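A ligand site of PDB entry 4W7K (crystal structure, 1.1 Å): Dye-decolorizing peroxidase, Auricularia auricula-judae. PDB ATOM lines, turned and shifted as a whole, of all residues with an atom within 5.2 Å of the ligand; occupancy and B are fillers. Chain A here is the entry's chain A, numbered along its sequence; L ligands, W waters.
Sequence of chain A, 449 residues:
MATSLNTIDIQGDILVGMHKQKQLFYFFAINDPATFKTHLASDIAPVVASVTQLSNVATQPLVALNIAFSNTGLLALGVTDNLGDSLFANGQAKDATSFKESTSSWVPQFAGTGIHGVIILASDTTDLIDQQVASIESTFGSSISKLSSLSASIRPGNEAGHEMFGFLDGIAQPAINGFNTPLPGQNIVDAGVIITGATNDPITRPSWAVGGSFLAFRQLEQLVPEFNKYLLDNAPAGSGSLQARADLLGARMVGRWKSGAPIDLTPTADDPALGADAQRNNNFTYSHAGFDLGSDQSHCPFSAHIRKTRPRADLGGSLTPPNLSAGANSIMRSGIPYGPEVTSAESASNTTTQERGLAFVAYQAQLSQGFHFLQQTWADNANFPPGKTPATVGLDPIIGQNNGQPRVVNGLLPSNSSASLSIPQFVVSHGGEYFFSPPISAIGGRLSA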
ATOM      1  N   GLU A 163     -18.680  30.873   9.310  1.00  0.00           N
ATOM      2  CA  GLU A 163     -18.304  29.485   9.246  1.00  0.00           C
ATOM      3  C   GLU A 163     -16.788  29.381   8.973  1.00  0.00           C
ATOM      4  O   GLU A 163     -16.100  30.399   8.818  1.00  0.00           O
ATOM      5  CB  GLU A 163     -19.222  28.728   8.296  1.00  0.00           C
ATOM      6  CG  GLU A 163     -19.342  29.284   6.893  1.00  0.00           C
ATOM      7  CD  GLU A 163     -18.041  29.176   6.153  1.00  0.00           C
ATOM      8  OE1 GLU A 163     -17.555  30.208   5.653  1.00  0.00           O
ATOM      9  OE2 GLU A 163     -17.482  28.047   6.121  1.00  0.00           O
ATOM     10  N   PHE A 165     -14.819  28.576   6.501  1.00  0.00           N
ATOM     11  CA  PHE A 165     -14.193  29.198   5.324  1.00  0.00           C
ATOM     12  C   PHE A 165     -14.109  30.717   5.434  1.00  0.00           C
ATOM     13  O   PHE A 165     -13.510  31.375   4.592  1.00  0.00           O
ATOM     14  CB  PHE A 165     -14.961  28.885   4.024  1.00  0.00           C
ATOM     15  CG  PHE A 165     -14.899  27.454   3.563  1.00  0.00           C
ATOM     16  CD1 PHE A 165     -13.740  26.711   3.636  1.00  0.00           C
ATOM     17  CD2 PHE A 165     -16.019  26.853   3.008  1.00  0.00           C
ATOM     18  CE1 PHE A 165     -13.711  25.386   3.204  1.00  0.00           C
ATOM     19  CE2 PHE A 165     -15.994  25.542   2.571  1.00  0.00           C
ATOM     20  CZ  PHE A 165     -14.847  24.805   2.676  1.00  0.00           C
ATOM     21  N   PHE A 167     -17.006  32.912   5.886  1.00  0.00           N
ATOM     22  CA  PHE A 167     -18.197  33.627   5.434  1.00  0.00           C
ATOM     23  C   PHE A 167     -19.201  33.774   6.552  1.00  0.00           C
ATOM     24  O   PHE A 167     -19.521  32.804   7.237  1.00  0.00           O
ATOM     25  CB  PHE A 167     -18.851  32.921   4.244  1.00  0.00           C
ATOM     26  CG  PHE A 167     -17.986  32.902   3.008  1.00  0.00           C
ATOM     27  CD1 PHE A 167     -16.917  32.034   2.896  1.00  0.00           C
ATOM     28  CD2 PHE A 167     -18.214  33.778   1.966  1.00  0.00           C
ATOM     29  CE1 PHE A 167     -16.096  32.046   1.776  1.00  0.00           C
ATOM     30  CE2 PHE A 167     -17.406  33.802   0.846  1.00  0.00           C
ATOM     31  CZ  PHE A 167     -16.334  32.948   0.750  1.00  0.00           C
ATOM     32  N   LEU A 168     -19.778  34.972   6.671  1.00  0.00           N
ATOM     33  CA  LEU A 168     -20.862  35.197   7.623  1.00  0.00           C
ATOM     34  C   LEU A 168     -22.000  34.234   7.284  1.00  0.00           C
ATOM     35  O   LEU A 168     -22.413  34.081   6.122  1.00  0.00           O
ATOM     36  CB  LEU A 168     -21.330  36.633   7.536  1.00  0.00           C
ATOM     37  CG  LEU A 168     -22.450  37.015   8.506  1.00  0.00           C
ATOM     38  CD1 LEU A 168     -22.004  36.847   9.965  1.00  0.00           C
ATOM     39  CD2 LEU A 168     -22.880  38.456   8.275  1.00  0.00           C
ATOM     40  N   ASP A 169     -22.483  33.551   8.302  1.00  0.00           N
ATOM     41  CA  ASP A 169     -23.505  32.554   8.134  1.00  0.00           C
ATOM     42  C   ASP A 169     -24.713  32.921   8.991  1.00  0.00           C
ATOM     43  O   ASP A 169     -24.655  33.800   9.841  1.00  0.00           O
ATOM     44  CB  ASP A 169     -22.896  31.197   8.506  1.00  0.00           C
ATOM     45  CG  ASP A 169     -23.754  30.012   8.099  1.00  0.00           C
ATOM     46  OD1 ASP A 169     -24.699  30.156   7.264  1.00  0.00           O
ATOM     47  OD2 ASP A 169     -23.456  28.902   8.623  1.00  0.00           O
ATOM     48  N   GLY A 170     -25.826  32.249   8.743  1.00  0.00           N
ATOM     49  CA  GLY A 170     -27.026  32.490   9.515  1.00  0.00           C
ATOM     50  C   GLY A 170     -27.813  33.730   9.116  1.00  0.00           C
ATOM     51  O   GLY A 170     -28.649  34.217   9.873  1.00  0.00           O
ATOM     52  N   ILE A 171     -27.555  34.243   7.924  1.00  0.00           N
ATOM     53  CA  ILE A 171     -28.224  35.426   7.425  1.00  0.00           C
ATOM     54  C   ILE A 171     -29.640  35.067   6.966  1.00  0.00           C
ATOM     55  O   ILE A 171     -30.614  35.731   7.344  1.00  0.00           O
ATOM     56  CB  ILE A 171     -27.445  36.033   6.247  1.00  0.00           C
ATOM     57  CG1 ILE A 171     -26.084  36.537   6.726  1.00  0.00           C
ATOM     58  CG2 ILE A 171     -28.244  37.156   5.608  1.00  0.00           C
ATOM     59  CD1 ILE A 171     -25.134  36.866   5.606  1.00  0.00           C
ATOM     60  N   ALA A 172     -29.740  34.046   6.127  1.00  0.00           N
ATOM     61  CA  ALA A 172     -30.963  33.760   5.420  1.00  0.00           C
ATOM     62  C   ALA A 172     -31.720  32.563   6.005  1.00  0.00           C
ATOM     63  O   ALA A 172     -31.206  31.455   6.108  1.00  0.00           O
ATOM     64  CB  ALA A 172     -30.648  33.495   3.957  1.00  0.00           C
ATOM     65  N   GLN A 173     -32.971  32.814   6.365  1.00  0.00           N
ATOM     66  CA  GLN A 173     -33.884  31.784   6.869  1.00  0.00           C
ATOM     67  C   GLN A 173     -35.255  32.082   6.297  1.00  0.00           C
ATOM     68  O   GLN A 173     -35.582  33.247   6.048  1.00  0.00           O
ATOM     69  CB  GLN A 173     -34.002  31.832   8.407  1.00  0.00           C
ATOM     70  CG  GLN A 173     -32.683  31.749   9.148  1.00  0.00           C
ATOM     71  CD  GLN A 173     -32.082  30.384   9.260  1.00  0.00           C
ATOM     72  OE1 GLN A 173     -32.457  29.403   8.591  1.00  0.00           O
ATOM     73  NE2 GLN A 173     -31.041  30.319  10.080  1.00  0.00           N
ATOM     74  N   LEU A 220     -19.901  17.897   8.560  1.00  0.00           N
ATOM     75  CA  LEU A 220     -19.310  18.295   7.269  1.00  0.00           C
ATOM     76  C   LEU A 220     -17.943  18.898   7.497  1.00  0.00           C
ATOM     77  O   LEU A 220     -17.824  20.047   7.915  1.00  0.00           O
ATOM     78  CB  LEU A 220     -20.248  19.268   6.537  1.00  0.00           C
ATOM     79  CG  LEU A 220     -21.625  18.700   6.235  1.00  0.00           C
ATOM     80  CD1 LEU A 220     -22.480  19.739   5.534  1.00  0.00           C
ATOM     81  CD2 LEU A 220     -21.522  17.436   5.410  1.00  0.00           C
ATOM     82  N   GLN A 222     -14.525  20.673   6.596  1.00  0.00           N
ATOM     83  CA  GLN A 222     -14.118  21.687   5.647  1.00  0.00           C
ATOM     84  C   GLN A 222     -12.604  21.704   5.538  1.00  0.00           C
ATOM     85  O   GLN A 222     -11.890  21.740   6.531  1.00  0.00           O
ATOM     86  CB  GLN A 222     -14.649  23.040   6.068  1.00  0.00           C
ATOM     87  CG  GLN A 222     -16.156  23.113   5.991  1.00  0.00           C
ATOM     88  CD  GLN A 222     -16.713  24.368   6.566  1.00  0.00           C
ATOM     89  OE1 GLN A 222     -17.329  24.342   7.617  1.00  0.00           O
ATOM     90  NE2 GLN A 222     -16.565  25.464   5.860  1.00  0.00           N
ATOM     91  N   VAL A 254     -19.872  31.136  -3.267  1.00  0.00           N
ATOM     92  CA  VAL A 254     -20.867  31.099  -2.204  1.00  0.00           C
ATOM     93  C   VAL A 254     -22.133  31.808  -2.627  1.00  0.00           C
ATOM     94  O   VAL A 254     -23.249  31.378  -2.276  1.00  0.00           O
ATOM     95  CB  VAL A 254     -20.279  31.718  -0.908  1.00  0.00           C
ATOM     96  CG1 VAL A 254     -21.355  31.893   0.170  1.00  0.00           C
ATOM     97  CG2 VAL A 254     -19.137  30.860  -0.397  1.00  0.00           C
ATOM     98  N   ARG A 256     -22.248  35.091  -1.677  1.00  0.00           N
ATOM     99  CA  ARG A 256     -22.038  36.248  -0.810  1.00  0.00           C
ATOM    100  C   ARG A 256     -20.547  36.420  -0.600  1.00  0.00           C
ATOM    101  O   ARG A 256     -19.806  35.467  -0.590  1.00  0.00           O
ATOM    102  CB  ARG A 256     -22.667  36.010   0.561  1.00  0.00           C
ATOM    103  CG  ARG A 256     -24.182  35.853   0.546  1.00  0.00           C
ATOM    104  CD  ARG A 256     -24.706  35.749   1.994  1.00  0.00           C
ATOM    105  NE  ARG A 256     -26.156  35.609   1.995  1.00  0.00           N
ATOM    106  CZ  ARG A 256     -27.006  36.614   1.914  1.00  0.00           C
ATOM    107  NH1 ARG A 256     -26.565  37.877   1.942  1.00  0.00           N
ATOM    108  NH2 ARG A 256     -28.288  36.372   1.773  1.00  0.00           N
ATOM    109  N   ASN A 282     -30.566  40.732   2.176  1.00  0.00           N
ATOM    110  CA  ASN A 282     -31.319  39.639   1.590  1.00  0.00           C
ATOM    111  C   ASN A 282     -32.292  40.108   0.541  1.00  0.00           C
ATOM    112  O   ASN A 282     -33.063  39.325   0.025  1.00  0.00           O
ATOM    113  CB  ASN A 282     -32.021  38.789   2.657  1.00  0.00           C
ATOM    114  CG  ASN A 282     -32.027  37.320   2.290  1.00  0.00           C
ATOM    115  OD1 ASN A 282     -31.236  36.881   1.455  1.00  0.00           O
ATOM    116  ND2 ASN A 282     -32.931  36.560   2.857  1.00  0.00           N
ATOM    117  N   TYR A 286     -32.347  37.572  -7.788  1.00  0.00           N
ATOM    118  CA  TYR A 286     -31.508  37.178  -8.941  1.00  0.00           C
ATOM    119  C   TYR A 286     -31.942  37.780 -10.260  1.00  0.00           C
ATOM    120  O   TYR A 286     -31.202  37.692 -11.228  1.00  0.00           O
ATOM    121  CB  TYR A 286     -31.313  35.645  -9.091  1.00  0.00           C
ATOM    122  CG  TYR A 286     -30.662  35.033  -7.868  1.00  0.00           C
ATOM    123  CD1 TYR A 286     -29.451  35.498  -7.415  1.00  0.00           C
ATOM    124  CD2 TYR A 286     -31.283  34.012  -7.151  1.00  0.00           C
ATOM    125  CE1 TYR A 286     -28.857  34.971  -6.281  1.00  0.00           C
ATOM    126  CE2 TYR A 286     -30.695  33.488  -6.002  1.00  0.00           C
ATOM    127  CZ  TYR A 286     -29.496  34.001  -5.556  1.00  0.00           C
ATOM    128  OH  TYR A 286     -28.886  33.519  -4.444  1.00  0.00           O
ATOM    129  N   HIS A 305     -23.586  28.695  -4.339  1.00  0.00           N
ATOM    130  CA  HIS A 305     -24.221  27.904  -3.295  1.00  0.00           C
ATOM    131  C   HIS A 305     -25.621  28.403  -2.910  1.00  0.00           C
ATOM    132  O   HIS A 305     -26.557  27.626  -2.881  1.00  0.00           O
ATOM    133  CB  HIS A 305     -23.293  27.848  -2.093  1.00  0.00           C
ATOM    134  CG  HIS A 305     -23.889  27.145  -0.907  1.00  0.00           C
ATOM    135  ND1 HIS A 305     -24.393  25.866  -0.976  1.00  0.00           N
ATOM    136  CD2 HIS A 305     -24.027  27.525   0.381  1.00  0.00           C
ATOM    137  CE1 HIS A 305     -24.816  25.498   0.223  1.00  0.00           C
ATOM    138  NE2 HIS A 305     -24.613  26.489   1.063  1.00  0.00           N
ATOM    139  N   ILE A 306     -25.761  29.689  -2.614  1.00  0.00           N
ATOM    140  CA  ILE A 306     -27.059  30.165  -2.128  1.00  0.00           C
ATOM    141  C   ILE A 306     -28.102  30.157  -3.230  1.00  0.00           C
ATOM    142  O   ILE A 306     -29.292  30.010  -2.964  1.00  0.00           O
ATOM    143  CB  ILE A 306     -26.998  31.526  -1.398  1.00  0.00           C
ATOM    144  CG1 ILE A 306     -26.540  32.668  -2.308  1.00  0.00           C
ATOM    145  CG2 ILE A 306     -26.135  31.415  -0.134  1.00  0.00           C
ATOM    146  CD1 ILE A 306     -26.930  33.996  -1.733  1.00  0.00           C
ATOM    147  N   THR A 309     -29.391  26.605  -3.431  1.00  0.00           N
ATOM    148  CA  THR A 309     -30.167  26.172  -2.268  1.00  0.00           C
ATOM    149  C   THR A 309     -31.424  26.992  -2.004  1.00  0.00           C
ATOM    150  O   THR A 309     -32.349  26.474  -1.385  1.00  0.00           O
ATOM    151  CB  THR A 309     -29.326  26.053  -1.011  1.00  0.00           C
ATOM    152  OG1 THR A 309     -28.805  27.337  -0.723  1.00  0.00           O
ATOM    153  CG2 THR A 309     -28.207  25.022  -1.174  1.00  0.00           C
ATOM    154  N   ARG A 310     -31.478  28.228  -2.489  1.00  0.00           N
ATOM    155  CA  ARG A 310     -32.730  28.985  -2.577  1.00  0.00           C
ATOM    156  C   ARG A 310     -32.752  29.692  -3.915  1.00  0.00           C
ATOM    157  O   ARG A 310     -32.198  30.783  -4.073  1.00  0.00           O
ATOM    158  CB  ARG A 310     -32.923  29.990  -1.433  1.00  0.00           C
ATOM    159  CG  ARG A 310     -34.275  30.705  -1.557  1.00  0.00           C
ATOM    160  CD  ARG A 310     -34.454  31.897  -0.615  1.00  0.00           C
ATOM    161  NE  ARG A 310     -35.674  32.614  -0.959  1.00  0.00           N
ATOM    162  CZ  ARG A 310     -35.913  33.890  -0.674  1.00  0.00           C
ATOM    163  NH1 ARG A 310     -35.105  34.605   0.077  1.00  0.00           N
ATOM    164  NH2 ARG A 310     -37.009  34.473  -1.145  1.00  0.00           N
ATOM    165  N   ARG A 312     -34.892  31.281  -5.720  1.00  0.00           N
ATOM    166  CA  ARG A 312     -35.613  32.550  -5.897  1.00  0.00           C
ATOM    167  C   ARG A 312     -36.204  32.620  -7.305  1.00  0.00           C
ATOM    168  O   ARG A 312     -36.927  31.699  -7.693  1.00  0.00           O
ATOM    169  CB  ARG A 312     -34.750  33.763  -5.525  1.00  0.00           C
ATOM    170  CG  ARG A 312     -34.155  33.671  -4.117  1.00  0.00           C
ATOM    171  CD  ARG A 312     -33.420  34.936  -3.679  1.00  0.00           C
ATOM    172  NE  ARG A 312     -32.617  34.600  -2.508  1.00  0.00           N
ATOM    173  CZ  ARG A 312     -32.396  35.405  -1.467  1.00  0.00           C
ATOM    174  NH1 ARG A 312     -32.866  36.634  -1.426  1.00  0.00           N
ATOM    175  NH2 ARG A 312     -31.685  34.953  -0.454  1.00  0.00           N
ATOM    176  N   ILE A 331     -35.653  25.390   4.461  1.00  0.00           N
ATOM    177  CA  ILE A 331     -35.126  24.790   5.672  1.00  0.00           C
ATOM    178  C   ILE A 331     -34.712  25.857   6.648  1.00  0.00           C
ATOM    179  O   ILE A 331     -34.274  26.933   6.259  1.00  0.00           O
ATOM    180  CB  ILE A 331     -33.911  23.844   5.367  1.00  0.00           C
ATOM    181  CG1 ILE A 331     -32.715  24.575   4.722  1.00  0.00           C
ATOM    182  CG2 ILE A 331     -34.361  22.672   4.510  1.00  0.00           C
ATOM    183  CD1 ILE A 331     -31.468  23.715   4.633  1.00  0.00           C
ATOM    184  N   ARG A 333     -31.920  26.641   9.351  1.00  0.00           N
ATOM    185  CA  ARG A 333     -30.567  26.184   9.607  1.00  0.00           C
ATOM    186  C   ARG A 333     -30.087  26.652  10.973  1.00  0.00           C
ATOM    187  O   ARG A 333     -30.187  27.845  11.303  1.00  0.00           O
ATOM    188  CB  ARG A 333     -29.624  26.671   8.529  1.00  0.00           C
ATOM    189  CG  ARG A 333     -29.917  26.084   7.171  1.00  0.00           C
ATOM    190  CD  ARG A 333     -29.020  26.631   6.058  1.00  0.00           C
ATOM    191  NE  ARG A 333     -29.215  28.066   5.950  1.00  0.00           N
ATOM    192  CZ  ARG A 333     -28.286  28.995   6.089  1.00  0.00           C
ATOM    193  NH1 ARG A 333     -27.004  28.671   6.272  1.00  0.00           N
ATOM    194  NH2 ARG A 333     -28.663  30.252   6.104  1.00  0.00           N
ATOM    195  N   LEU A 358     -18.354  22.184   9.743  1.00  0.00           N
ATOM    196  CA  LEU A 358     -19.677  22.629  10.130  1.00  0.00           C
ATOM    197  C   LEU A 358     -20.478  21.479  10.708  1.00  0.00           C
ATOM    198  O   LEU A 358     -20.621  20.443  10.058  1.00  0.00           O
ATOM    199  CB  LEU A 358     -20.415  23.220   8.921  1.00  0.00           C
ATOM    200  CG  LEU A 358     -21.772  23.842   9.217  1.00  0.00           C
ATOM    201  CD1 LEU A 358     -21.640  25.069  10.115  1.00  0.00           C
ATOM    202  CD2 LEU A 358     -22.514  24.178   7.937  1.00  0.00           C
ATOM    203  N   PHE A 360     -23.674  20.734  10.793  1.00  0.00           N
ATOM    204  CA  PHE A 360     -24.815  21.217  10.023  1.00  0.00           C
ATOM    205  C   PHE A 360     -26.107  20.681  10.622  1.00  0.00           C
ATOM    206  O   PHE A 360     -26.216  19.480  10.861  1.00  0.00           O
ATOM    207  CB  PHE A 360     -24.646  20.786   8.568  1.00  0.00           C
ATOM    208  CG  PHE A 360     -25.836  21.065   7.686  1.00  0.00           C
ATOM    209  CD1 PHE A 360     -26.867  20.152   7.574  1.00  0.00           C
ATOM    210  CD2 PHE A 360     -25.945  22.251   7.000  1.00  0.00           C
ATOM    211  CE1 PHE A 360     -27.972  20.405   6.774  1.00  0.00           C
ATOM    212  CE2 PHE A 360     -27.066  22.510   6.187  1.00  0.00           C
ATOM    213  CZ  PHE A 360     -28.052  21.588   6.075  1.00  0.00           C
ATOM    214  N   PHE A 371     -33.734  19.333   3.354  1.00  0.00           N
ATOM    215  CA  PHE A 371     -32.336  18.990   3.196  1.00  0.00           C
ATOM    216  C   PHE A 371     -32.070  17.991   2.048  1.00  0.00           C
ATOM    217  O   PHE A 371     -31.187  18.204   1.209  1.00  0.00           O
ATOM    218  CB  PHE A 371     -31.751  18.423   4.504  1.00  0.00           C
ATOM    219  CG  PHE A 371     -30.467  17.649   4.286  1.00  0.00           C
ATOM    220  CD1 PHE A 371     -29.300  18.307   3.903  1.00  0.00           C
ATOM    221  CD2 PHE A 371     -30.466  16.272   4.325  1.00  0.00           C
ATOM    222  CE1 PHE A 371     -28.155  17.603   3.599  1.00  0.00           C
ATOM    223  CE2 PHE A 371     -29.330  15.556   4.019  1.00  0.00           C
ATOM    224  CZ  PHE A 371     -28.176  16.217   3.631  1.00  0.00           C
ATOM    225  N   LEU A 374     -32.631  19.618  -1.456  1.00  0.00           N
ATOM    226  CA  LEU A 374     -31.634  20.639  -1.775  1.00  0.00           C
ATOM    227  C   LEU A 374     -30.334  19.975  -2.173  1.00  0.00           C
ATOM    228  O   LEU A 374     -29.667  20.397  -3.118  1.00  0.00           O
ATOM    229  CB  LEU A 374     -31.413  21.565  -0.595  1.00  0.00           C
ATOM    230  CG  LEU A 374     -32.344  22.785  -0.529  1.00  0.00           C
ATOM    231  CD1 LEU A 374     -33.814  22.466  -0.734  1.00  0.00           C
ATOM    232  CD2 LEU A 374     -32.115  23.533   0.766  1.00  0.00           C
ATOM    233  N   GLN A 375     -29.934  18.941  -1.455  1.00  0.00           N
ATOM    234  CA  GLN A 375     -28.670  18.273  -1.733  1.00  0.00           C
ATOM    235  C   GLN A 375     -28.741  17.520  -3.073  1.00  0.00           C
ATOM    236  O   GLN A 375     -27.891  17.681  -3.946  1.00  0.00           O
ATOM    237  CB  GLN A 375     -28.288  17.340  -0.582  1.00  0.00           C
ATOM    238  CG  GLN A 375     -26.914  16.687  -0.745  1.00  0.00           C
ATOM    239  CD  GLN A 375     -25.772  17.643  -0.529  1.00  0.00           C
ATOM    240  OE1 GLN A 375     -25.684  18.262   0.516  1.00  0.00           O
ATOM    241  NE2 GLN A 375     -24.901  17.773  -1.520  1.00  0.00           N
ATOM    242  N   ILE A 398     -19.657  24.494  -3.163  1.00  0.00           N
ATOM    243  CA  ILE A 398     -19.465  24.308  -1.736  1.00  0.00           C
ATOM    244  C   ILE A 398     -19.866  22.902  -1.305  1.00  0.00           C
ATOM    245  O   ILE A 398     -19.080  22.218  -0.632  1.00  0.00           O
ATOM    246  CB  ILE A 398     -20.215  25.408  -0.928  1.00  0.00           C
ATOM    247  CG1 ILE A 398     -19.761  26.812  -1.394  1.00  0.00           C
ATOM    248  CG2 ILE A 398     -19.999  25.230   0.576  1.00  0.00           C
ATOM    249  CD1 ILE A 398     -18.248  27.087  -1.347  1.00  0.00           C
ATOM    250  N   ILE A 399     -21.083  22.475  -1.655  1.00  0.00           N
ATOM    251  CA  ILE A 399     -21.619  21.209  -1.160  1.00  0.00           C
ATOM    252  C   ILE A 399     -21.891  20.162  -2.210  1.00  0.00           C
ATOM    253  O   ILE A 399     -22.275  19.057  -1.870  1.00  0.00           O
ATOM    254  CB  ILE A 399     -22.908  21.414  -0.321  1.00  0.00           C
ATOM    255  CG1 ILE A 399     -24.049  21.998  -1.162  1.00  0.00           C
ATOM    256  CG2 ILE A 399     -22.607  22.278   0.904  1.00  0.00           C
ATOM    257  CD1 ILE A 399     -25.422  21.856  -0.533  1.00  0.00           C
ATOM    258  N   VAL A 427     -15.589  20.318   1.014  1.00  0.00           N
ATOM    259  CA  VAL A 427     -16.438  19.863   2.104  1.00  0.00           C
ATOM    260  C   VAL A 427     -16.547  18.348   1.983  1.00  0.00           C
ATOM    261  O   VAL A 427     -16.841  17.830   0.894  1.00  0.00           O
ATOM    262  CB  VAL A 427     -17.832  20.496   2.030  1.00  0.00           C
ATOM    263  CG1 VAL A 427     -18.753  19.908   3.111  1.00  0.00           C
ATOM    264  CG2 VAL A 427     -17.721  21.989   2.175  1.00  0.00           C
HETATM  265  C1  LIG L   1     -26.512  29.650   3.002  1.00  0.00           C
HETATM  266  C2  LIG L   1     -22.101  27.912   3.960  1.00  0.00           C
HETATM  267  C3  LIG L   1     -23.885  23.367   3.926  1.00  0.00           C
HETATM  268  C4  LIG L   1     -28.206  25.105   2.588  1.00  0.00           C
HETATM  269  C5  LIG L   1     -25.165  29.565   3.270  1.00  0.00           C
HETATM  270  C6  LIG L   1     -24.262  30.685   3.380  1.00  0.00           C
HETATM  271  C7  LIG L   1     -23.040  30.207   3.646  1.00  0.00           C
HETATM  272  C8  LIG L   1     -23.138  28.778   3.715  1.00  0.00           C
HETATM  273  C9  LIG L   1     -21.723  30.969   3.887  1.00  0.00           C
HETATM  274  C10 LIG L   1     -24.655  32.165   3.188  1.00  0.00           C
HETATM  275  C11 LIG L   1     -25.143  32.716   4.526  1.00  0.00           C
HETATM  276  C12 LIG L   1     -26.632  32.888   4.501  1.00  0.00           C
HETATM  277  O1  LIG L   1     -27.173  33.193   3.394  1.00  0.00           O
HETATM  278  O2  LIG L   1     -27.258  32.710   5.591  1.00  0.00           O
HETATM  279  C13 LIG L   1     -22.178  26.528   4.052  1.00  0.00           C
HETATM  280  C14 LIG L   1     -21.104  25.611   4.316  1.00  0.00           C
HETATM  281  C15 LIG L   1     -21.606  24.377   4.315  1.00  0.00           C
HETATM  282  C16 LIG L   1     -23.009  24.446   4.028  1.00  0.00           C
HETATM  283  C17 LIG L   1     -19.643  26.037   4.528  1.00  0.00           C
HETATM  284  C18 LIG L   1     -20.862  23.052   4.563  1.00  0.00           C
HETATM  285  C19 LIG L   1     -19.764  22.958   5.309  1.00  0.00           C
HETATM  286  C20 LIG L   1     -25.195  23.444   3.473  1.00  0.00           C
HETATM  287  C21 LIG L   1     -26.029  22.313   3.140  1.00  0.00           C
HETATM  288  C22 LIG L   1     -27.210  22.792   2.739  1.00  0.00           C
HETATM  289  C23 LIG L   1     -27.161  24.241   2.830  1.00  0.00           C
HETATM  290  C24 LIG L   1     -25.603  20.840   3.275  1.00  0.00           C
HETATM  291  C25 LIG L   1     -28.429  22.061   2.259  1.00  0.00           C
HETATM  292  C26 LIG L   1     -28.404  20.861   1.662  1.00  0.00           C
HETATM  293  C27 LIG L   1     -28.174  26.496   2.660  1.00  0.00           C
HETATM  294  C28 LIG L   1     -29.318  27.348   2.501  1.00  0.00           C
HETATM  295  C29 LIG L   1     -28.796  28.708   2.611  1.00  0.00           C
HETATM  296  C30 LIG L   1     -27.387  28.577   2.843  1.00  0.00           C
HETATM  297  C31 LIG L   1     -30.767  26.970   2.259  1.00  0.00           C
HETATM  298  C32 LIG L   1     -29.625  29.968   2.488  1.00  0.00           C
HETATM  299  C33 LIG L   1     -29.991  30.243   1.045  1.00  0.00           C
HETATM  300  C34 LIG L   1     -30.918  31.434   0.942  1.00  0.00           C
HETATM  301  O3  LIG L   1     -30.603  32.341   0.135  1.00  0.00           O
HETATM  302  O4  LIG L   1     -31.971  31.455   1.631  1.00  0.00           O
HETATM  303  N1  LIG L   1     -24.440  28.406   3.497  1.00  0.00           N
HETATM  304  N2  LIG L   1     -23.339  25.773   3.903  1.00  0.00           N
HETATM  305  N3  LIG L   1     -25.902  24.616   3.245  1.00  0.00           N
HETATM  306  N4  LIG L   1     -27.065  27.244   2.910  1.00  0.00           N
HETATM  307 FE1  LIG L   1     -25.137  26.505   3.111  1.00  0.00          FE
HETATM  308  O   HOH W   1     -33.270  29.858   3.426  1.00  0.00           O
HETATM  309  O   HOH W   2     -30.699  32.532  -2.666  1.00  0.00           O
HETATM  310  O   HOH W   3     -28.483  33.641   1.330  1.00  0.00           O
HETATM  311  O   HOH W   4     -33.365  33.736   2.082  1.00  0.00           O
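A ring nitrogen (NE2) of His 305 binds an iron atom (FE1) of the ligand, 2.1 Å away. N of Ile 171 sits at hydrogen-bond distance from O2 of the ligand (2.8 Å). An oxygen (O2) of the ligand lies within salt-bridge range of the guanidinium group of Arg 333 (2.9 Å). An oxygen (O2) of the ligand is in hydrogen-bond range of the backbone NH (N) of Gly 170. An oxygen (O3) of the ligand is in salt-bridge range of the guanidinium group (NH2) of Arg 312, 2.9 Å away. N of Ala 172 lies within hydrogen-bond range of O2 of the ligand (2.9 Å). The guanidinium group (NE) of Arg 256 is in salt-bridge range of an oxygen (O1) of the ligand.
O of Ile 399 is in hydrogen-bond range of NE2 of Gln 375. The guanidinium group of Arg 333 lies within salt-bridge range of the side-chain carboxylate of Asp 169, at 2.9 Å. The backbone NH of His 305 sits at hydrogen-bond distance from the backbone carbonyl oxygen of Val 254, 3.4 Å away. NE2 of Gln 173 lies within hydrogen-bond range of O of Arg 333 (2.9 Å). NH2 of Arg 312 sits at hydrogen-bond distance from OD1 of Asn 282 (2.8 Å). The backbone NH (N) of Phe 167 is in hydrogen-bond range of the side-chain carboxylate (OE1) of Glu 163 (2.8 Å). The side-chain carboxylate (OE2) of Glu 163 sits at hydrogen-bond distance from the side-chain amide nitrogen (NE2) of Gln 222. The side-chain amide oxygen (OE1) of Gln 222 lies within hydrogen-bond range of the backbone NH (N) of Leu 358, at 3.2 Å.
Residues that only touch the ligand: Phe 360 (3.2 Å), Thr 309 (3.3 Å), Glu 163 (3.4 Å), Arg 310 (3.4 Å), Gln 222 (3.4 Å), Leu 168 (3.4 Å), Ile 399 (3.5 Å), Phe 167 (3.5 Å), Phe 371 (3.5 Å), Ile 306 (3.6 Å), Leu 358 (3.7 Å), Asp 169 (3.8 Å), Gln 375 (3.8 Å), Leu 220 (3.8 Å), Leu 374 (3.8 Å), Val 254 (3.8 Å), Val 427 (3.9 Å), Ile 398 (3.9 Å) and Ile 331 (3.9 Å). Hydrophobic or aromatic side chains that line the ligand: Phe 167, Ile 171, Ala 172, Leu 220, Val 254, His 305, Ile 306, Ile 331, Leu 358, Phe 360, Phe 371, Leu 374, Ile 398, Ile 399 and Val 427. 26 residues have an atom within 4 Å of the ligand: Glu 163, Phe 167, Leu 168, Asp 169, Gly 170, Ile 171, Ala 172, Leu 220, Gln 222, Val 254, Arg 256, His 305, Ile 306, Thr 309, Arg 310, Arg 312, Ile 331, Arg 333, Leu 358, Phe 360, Phe 371, Leu 374, Gln 375, Ile 398, Ile 399 and Val 427.
Water W3 bridges an oxygen (O1) of the ligand (2.5 Å) and the guanidinium group of Arg 256 (2.8 Å). Water W2 lies within hydrogen-bond range of O of Arg 310, OH of Tyr 286, O3 of the ligand, NE of Arg 312 and O of Ile 306.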
